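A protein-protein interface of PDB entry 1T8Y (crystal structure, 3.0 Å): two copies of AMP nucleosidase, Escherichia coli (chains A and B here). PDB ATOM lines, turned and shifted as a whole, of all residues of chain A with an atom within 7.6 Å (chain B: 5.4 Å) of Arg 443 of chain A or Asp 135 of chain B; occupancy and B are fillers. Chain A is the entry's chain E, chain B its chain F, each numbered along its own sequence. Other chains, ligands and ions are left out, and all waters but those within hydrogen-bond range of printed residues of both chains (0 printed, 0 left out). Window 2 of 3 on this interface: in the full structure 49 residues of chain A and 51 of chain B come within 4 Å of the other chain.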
ATOM      1  N   ARG A 208      19.777  18.770   7.291  1.00  0.00           N
ATOM      2  CA  ARG A 208      20.328  19.995   6.731  1.00  0.00           C
ATOM      3  C   ARG A 208      21.308  20.734   7.643  1.00  0.00           C
ATOM      4  O   ARG A 208      21.993  21.653   7.197  1.00  0.00           O
ATOM      5  CB  ARG A 208      19.202  20.954   6.323  1.00  0.00           C
ATOM      6  CG  ARG A 208      18.609  20.712   4.926  1.00  0.00           C
ATOM      7  CD  ARG A 208      18.462  22.044   4.189  1.00  0.00           C
ATOM      8  NE  ARG A 208      19.739  22.759   4.188  1.00  0.00           N
ATOM      9  CZ  ARG A 208      19.877  24.081   4.269  1.00  0.00           C
ATOM     10  NH1 ARG A 208      18.803  24.859   4.353  1.00  0.00           N
ATOM     11  NH2 ARG A 208      21.092  24.624   4.297  1.00  0.00           N
ATOM     12  N   ILE A 315       7.723  31.595  12.253  1.00  0.00           N
ATOM     13  CA  ILE A 315       8.641  30.564  11.801  1.00  0.00           C
ATOM     14  C   ILE A 315      10.015  31.201  11.590  1.00  0.00           C
ATOM     15  O   ILE A 315      10.137  32.256  10.968  1.00  0.00           O
ATOM     16  CB  ILE A 315       8.146  29.905  10.487  1.00  0.00           C
ATOM     17  CG1 ILE A 315       6.854  29.143  10.767  1.00  0.00           C
ATOM     18  CG2 ILE A 315       9.211  28.976   9.924  1.00  0.00           C
ATOM     19  CD1 ILE A 315       6.396  28.288   9.650  1.00  0.00           C
ATOM     20  N   GLU A 434      -0.598  26.459  10.197  1.00  0.00           N
ATOM     21  CA  GLU A 434       0.637  26.241   9.471  1.00  0.00           C
ATOM     22  C   GLU A 434       1.519  25.101   9.997  1.00  0.00           C
ATOM     23  O   GLU A 434       2.409  25.312  10.827  1.00  0.00           O
ATOM     24  CB  GLU A 434       1.419  27.551   9.447  1.00  0.00           C
ATOM     25  CG  GLU A 434       2.710  27.492   8.673  1.00  0.00           C
ATOM     26  CD  GLU A 434       3.239  28.877   8.358  1.00  0.00           C
ATOM     27  OE1 GLU A 434       3.358  29.701   9.299  1.00  0.00           O
ATOM     28  OE2 GLU A 434       3.536  29.137   7.168  1.00  0.00           O
ATOM     29  N   LYS A 436       4.243  22.703   8.852  1.00  0.00           N
ATOM     30  CA  LYS A 436       5.240  22.374   7.841  1.00  0.00           C
ATOM     31  C   LYS A 436       6.190  21.314   8.383  1.00  0.00           C
ATOM     32  O   LYS A 436       6.865  21.538   9.389  1.00  0.00           O
ATOM     33  CB  LYS A 436       6.034  23.631   7.471  1.00  0.00           C
ATOM     34  CG  LYS A 436       5.182  24.781   6.940  1.00  0.00           C
ATOM     35  CD  LYS A 436       6.027  26.022   6.678  1.00  0.00           C
ATOM     36  CE  LYS A 436       5.271  27.053   5.851  1.00  0.00           C
ATOM     37  NZ  LYS A 436       4.960  26.561   4.471  1.00  0.00           N
ATOM     38  N   GLN A 440      10.237  20.312   3.735  1.00  0.00           N
ATOM     39  CA  GLN A 440       9.237  20.830   2.817  1.00  0.00           C
ATOM     40  C   GLN A 440       9.530  22.291   2.505  1.00  0.00           C
ATOM     41  O   GLN A 440      10.422  22.892   3.102  1.00  0.00           O
ATOM     42  CB  GLN A 440       7.839  20.702   3.436  1.00  0.00           C
ATOM     43  CG  GLN A 440       7.336  19.279   3.543  1.00  0.00           C
ATOM     44  CD  GLN A 440       6.003  19.187   4.272  1.00  0.00           C
ATOM     45  OE1 GLN A 440       5.414  18.119   4.367  1.00  0.00           O
ATOM     46  NE2 GLN A 440       5.525  20.319   4.798  1.00  0.00           N
ATOM     47  N   ALA A 441       8.770  22.859   1.575  1.00  0.00           N
ATOM     48  CA  ALA A 441       8.944  24.253   1.171  1.00  0.00           C
ATOM     49  C   ALA A 441       8.799  25.232   2.336  1.00  0.00           C
ATOM     50  O   ALA A 441       8.085  26.242   2.243  1.00  0.00           O
ATOM     51  CB  ALA A 441       7.943  24.592   0.078  1.00  0.00           C
ATOM     52  N   ASN A 442       9.500  24.954   3.427  1.00  0.00           N
ATOM     53  CA  ASN A 442       9.437  25.830   4.573  1.00  0.00           C
ATOM     54  C   ASN A 442      10.401  26.983   4.406  1.00  0.00           C
ATOM     55  O   ASN A 442      11.501  26.985   4.953  1.00  0.00           O
ATOM     56  CB  ASN A 442       9.743  25.068   5.842  1.00  0.00           C
ATOM     57  CG  ASN A 442       9.374  25.849   7.062  1.00  0.00           C
ATOM     58  OD1 ASN A 442       8.908  26.990   6.965  1.00  0.00           O
ATOM     59  ND2 ASN A 442       9.575  25.251   8.225  1.00  0.00           N
ATOM     60  N   ARG A 443       9.955  27.964   3.636  1.00  0.00           N
ATOM     61  CA  ARG A 443      10.741  29.141   3.348  1.00  0.00           C
ATOM     62  C   ARG A 443      11.609  29.651   4.497  1.00  0.00           C
ATOM     63  O   ARG A 443      12.823  29.441   4.517  1.00  0.00           O
ATOM     64  CB  ARG A 443       9.809  30.260   2.883  1.00  0.00           C
ATOM     65  CG  ARG A 443      10.501  31.592   2.576  1.00  0.00           C
ATOM     66  CD  ARG A 443      10.737  31.774   1.086  1.00  0.00           C
ATOM     67  NE  ARG A 443      10.066  32.962   0.549  1.00  0.00           N
ATOM     68  CZ  ARG A 443      10.382  34.216   0.865  1.00  0.00           C
ATOM     69  NH1 ARG A 443      11.365  34.466   1.725  1.00  0.00           N
ATOM     70  NH2 ARG A 443       9.714  35.224   0.315  1.00  0.00           N
ATOM     71  N   PHE A 444      10.974  30.302   5.464  1.00  0.00           N
ATOM     72  CA  PHE A 444      11.691  30.935   6.576  1.00  0.00           C
ATOM     73  C   PHE A 444      12.475  30.089   7.587  1.00  0.00           C
ATOM     74  O   PHE A 444      13.351  30.614   8.288  1.00  0.00           O
ATOM     75  CB  PHE A 444      10.741  31.896   7.297  1.00  0.00           C
ATOM     76  CG  PHE A 444      10.116  32.907   6.381  1.00  0.00           C
ATOM     77  CD1 PHE A 444       8.971  32.590   5.649  1.00  0.00           C
ATOM     78  CD2 PHE A 444      10.712  34.156   6.196  1.00  0.00           C
ATOM     79  CE1 PHE A 444       8.431  33.502   4.743  1.00  0.00           C
ATOM     80  CE2 PHE A 444      10.178  35.080   5.289  1.00  0.00           C
ATOM     81  CZ  PHE A 444       9.037  34.751   4.561  1.00  0.00           C
ATOM     82  N   TYR A 445      12.173  28.798   7.676  1.00  0.00           N
ATOM     83  CA  TYR A 445      12.921  27.949   8.581  1.00  0.00           C
ATOM     84  C   TYR A 445      14.256  27.665   7.901  1.00  0.00           C
ATOM     85  O   TYR A 445      15.334  27.796   8.492  1.00  0.00           O
ATOM     86  CB  TYR A 445      12.185  26.636   8.837  1.00  0.00           C
ATOM     87  CG  TYR A 445      13.018  25.669   9.641  1.00  0.00           C
ATOM     88  CD1 TYR A 445      13.705  26.102  10.782  1.00  0.00           C
ATOM     89  CD2 TYR A 445      13.170  24.344   9.246  1.00  0.00           C
ATOM     90  CE1 TYR A 445      14.526  25.257  11.497  1.00  0.00           C
ATOM     91  CE2 TYR A 445      13.996  23.481   9.967  1.00  0.00           C
ATOM     92  CZ  TYR A 445      14.673  23.953  11.089  1.00  0.00           C
ATOM     93  OH  TYR A 445      15.519  23.133  11.794  1.00  0.00           O
ATOM     94  N   GLU A 446      14.160  27.289   6.633  1.00  0.00           N
ATOM     95  CA  GLU A 446      15.322  26.970   5.826  1.00  0.00           C
ATOM     96  C   GLU A 446      16.309  28.117   5.800  1.00  0.00           C
ATOM     97  O   GLU A 446      17.515  27.920   5.946  1.00  0.00           O
ATOM     98  CB  GLU A 446      14.880  26.644   4.410  1.00  0.00           C
ATOM     99  CG  GLU A 446      14.018  25.408   4.304  1.00  0.00           C
ATOM    100  CD  GLU A 446      14.754  24.162   4.726  1.00  0.00           C
ATOM    101  OE1 GLU A 446      15.975  24.071   4.467  1.00  0.00           O
ATOM    102  OE2 GLU A 446      14.108  23.265   5.309  1.00  0.00           O
ATOM    103  N   GLY A 447      15.798  29.319   5.610  1.00  0.00           N
ATOM    104  CA  GLY A 447      16.686  30.456   5.569  1.00  0.00           C
ATOM    105  C   GLY A 447      17.470  30.629   6.853  1.00  0.00           C
ATOM    106  O   GLY A 447      18.572  31.175   6.844  1.00  0.00           O
ATOM    107  N   ALA A 448      16.918  30.143   7.964  1.00  0.00           N
ATOM    108  CA  ALA A 448      17.567  30.305   9.267  1.00  0.00           C
ATOM    109  C   ALA A 448      18.573  29.223   9.669  1.00  0.00           C
ATOM    110  O   ALA A 448      19.572  29.512  10.336  1.00  0.00           O
ATOM    111  CB  ALA A 448      16.493  30.471  10.354  1.00  0.00           C
ATOM    112  N   ILE A 449      18.323  27.989   9.259  1.00  0.00           N
ATOM    113  CA  ILE A 449      19.213  26.897   9.618  1.00  0.00           C
ATOM    114  C   ILE A 449      20.686  27.298   9.748  1.00  0.00           C
ATOM    115  O   ILE A 449      21.325  27.001  10.761  1.00  0.00           O
ATOM    116  CB  ILE A 449      19.065  25.744   8.632  1.00  0.00           C
ATOM    117  CG1 ILE A 449      17.614  25.265   8.671  1.00  0.00           C
ATOM    118  CG2 ILE A 449      20.038  24.638   8.965  1.00  0.00           C
ATOM    119  CD1 ILE A 449      17.306  24.070   7.826  1.00  0.00           C
ATOM    120  N   THR B 133       5.731  29.231  -1.260  1.00  0.00           N
ATOM    121  CA  THR B 133       6.901  29.922  -0.747  1.00  0.00           C
ATOM    122  C   THR B 133       6.701  31.436  -0.753  1.00  0.00           C
ATOM    123  O   THR B 133       7.581  32.203  -1.145  1.00  0.00           O
ATOM    124  CB  THR B 133       8.125  29.553  -1.582  1.00  0.00           C
ATOM    125  OG1 THR B 133       7.705  29.251  -2.920  1.00  0.00           O
ATOM    126  CG2 THR B 133       8.831  28.349  -0.975  1.00  0.00           C
ATOM    127  N   LEU B 134       5.516  31.840  -0.316  1.00  0.00           N
ATOM    128  CA  LEU B 134       5.109  33.233  -0.206  1.00  0.00           C
ATOM    129  C   LEU B 134       5.872  33.919   0.916  1.00  0.00           C
ATOM    130  O   LEU B 134       6.360  33.258   1.825  1.00  0.00           O
ATOM    131  CB  LEU B 134       3.618  33.302   0.104  1.00  0.00           C
ATOM    132  CG  LEU B 134       2.630  33.004  -1.023  1.00  0.00           C
ATOM    133  CD1 LEU B 134       2.880  31.625  -1.620  1.00  0.00           C
ATOM    134  CD2 LEU B 134       1.225  33.116  -0.469  1.00  0.00           C
ATOM    135  N   ASP B 135       5.963  35.242   0.862  1.00  0.00           N
ATOM    136  CA  ASP B 135       6.675  35.987   1.890  1.00  0.00           C
ATOM    137  C   ASP B 135       5.866  35.994   3.177  1.00  0.00           C
ATOM    138  O   ASP B 135       4.873  35.288   3.290  1.00  0.00           O
ATOM    139  CB  ASP B 135       6.941  37.417   1.417  1.00  0.00           C
ATOM    140  CG  ASP B 135       5.669  38.209   1.188  1.00  0.00           C
ATOM    141  OD1 ASP B 135       5.100  38.725   2.173  1.00  0.00           O
ATOM    142  OD2 ASP B 135       5.237  38.314   0.023  1.00  0.00           O
ATOM    143  N   ARG B 136       6.289  36.788   4.149  1.00  0.00           N
ATOM    144  CA  ARG B 136       5.588  36.849   5.419  1.00  0.00           C
ATOM    145  C   ARG B 136       4.117  37.201   5.283  1.00  0.00           C
ATOM    146  O   ARG B 136       3.253  36.365   5.525  1.00  0.00           O
ATOM    147  CB  ARG B 136       6.260  37.859   6.336  1.00  0.00           C
ATOM    148  CG  ARG B 136       7.663  37.482   6.752  1.00  0.00           C
ATOM    149  CD  ARG B 136       7.671  36.270   7.652  1.00  0.00           C
ATOM    150  NE  ARG B 136       9.027  35.945   8.072  1.00  0.00           N
ATOM    151  CZ  ARG B 136       9.339  34.933   8.869  1.00  0.00           C
ATOM    152  NH1 ARG B 136       8.384  34.142   9.337  1.00  0.00           N
ATOM    153  NH2 ARG B 136      10.607  34.706   9.187  1.00  0.00           N
ATOM    154  N   SER B 137       3.836  38.443   4.904  1.00  0.00           N
ATOM    155  CA  SER B 137       2.463  38.917   4.748  1.00  0.00           C
ATOM    156  C   SER B 137       1.595  37.996   3.908  1.00  0.00           C
ATOM    157  O   SER B 137       0.458  37.716   4.267  1.00  0.00           O
ATOM    158  CB  SER B 137       2.461  40.304   4.129  1.00  0.00           C
ATOM    159  OG  SER B 137       3.253  41.175   4.906  1.00  0.00           O
ATOM    160  N   MET B 138       2.126  37.532   2.783  1.00  0.00           N
ATOM    161  CA  MET B 138       1.374  36.639   1.915  1.00  0.00           C
ATOM    162  C   MET B 138       0.883  35.415   2.659  1.00  0.00           C
ATOM    163  O   MET B 138      -0.252  34.983   2.463  1.00  0.00           O
ATOM    164  CB  MET B 138       2.223  36.207   0.719  1.00  0.00           C
ATOM    165  CG  MET B 138       2.239  37.227  -0.418  1.00  0.00           C
ATOM    166  SD  MET B 138       0.433  37.754  -1.038  1.00  0.00           S
ATOM    167  CE  MET B 138      -0.042  36.046  -1.951  1.00  0.00           C
ATOM    168  N   SER B 139       1.743  34.861   3.512  1.00  0.00           N
ATOM    169  CA  SER B 139       1.402  33.683   4.300  1.00  0.00           C
ATOM    170  C   SER B 139       0.354  34.041   5.336  1.00  0.00           C
ATOM    171  O   SER B 139      -0.702  33.411   5.412  1.00  0.00           O
ATOM    172  CB  SER B 139       2.643  33.134   5.003  1.00  0.00           C
ATOM    173  OG  SER B 139       3.574  32.614   4.068  1.00  0.00           O
ATOM    174  N   ALA B 140       0.652  35.058   6.132  1.00  0.00           N
ATOM    175  CA  ALA B 140      -0.267  35.499   7.161  1.00  0.00           C
ATOM    176  C   ALA B 140      -1.652  35.642   6.561  1.00  0.00           C
ATOM    177  O   ALA B 140      -2.633  35.150   7.119  1.00  0.00           O
ATOM    178  CB  ALA B 140       0.193  36.815   7.733  1.00  0.00           C
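O of Thr 133 of chain B lies within hydrogen-bond range of NE of Arg 443 of chain A.
The backbone carbonyl oxygen (O) of Ile 315 of chain A lies within hydrogen-bond range of the guanidinium group (NH1) of Arg 136 of chain B (3.0 Å).
Lys 436 of chain A touches none of the printed residues of chain B.
Arg 443 of chain A touches just these residues of chain B: Thr 133, Leu 134 and Asp 135.
Ala 448 of chain A touches none of the printed residues of chain B.
Printed residues of chain A within 4 Å of Thr 133 of chain B: Ala 441 (3.9 Å) and Arg 443 (3.1 Å).
Asp 135 of chain B touches just these residues of chain A: Arg 443 and Phe 444.
Printed residues of chain A within 4 Å of Arg 136 of chain B: Ile 315 and Phe 444.
The nearest residue of chain A that does not touch Asp 135 of chain B is Glu 434 of chain A (7.4 Å).
The nearest printed residue of chain A that does not touch Thr 133 of chain B is Asn 442 of chain A (5.6 Å).
No position is printed for both chains.
Of the 8 pairs that touch across the chains among the printed residues, none has its exchanged pair printed and touching as well.
Among the printed residues, merely in contact across the chains: Ala 441 of chain A with Thr 133 of chain B, Arg 443 of chain A with Leu 134 of chain B, Arg 443 of chain A with Asp 135 of chain B, Phe 444 of chain A with Leu 134 of chain B, Phe 444 of chain A with Asp 135 of chain B and Phe 444 of chain A with Arg 136 of chain B.
Of the 14 printed residues of chain A, 4 touch a printed residue of chain B.
Along chain B the printed residues that touch a printed residue of chain A span positions 133 to 136.
Among the printed residues, no Asp or Glu carboxylate lies within 4 Å of a Lys or Arg side-chain nitrogen of the other chain.
The side-chain hydroxyl (OG) of Ser 139 of chain B sits at hydrogen-bond distance from the backbone carbonyl oxygen (O) of Asp 135 of chain B (3.1 Å).
OD1 of Asp 135 of chain B sits at hydrogen-bond distance from N of Met 138 of chain B (3.3 Å).
The side-chain carboxylate (OD1) of Asp 135 of chain B lies within hydrogen-bond range of the backbone NH (N) of Ser 137 of chain B, 3.0 Å away.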
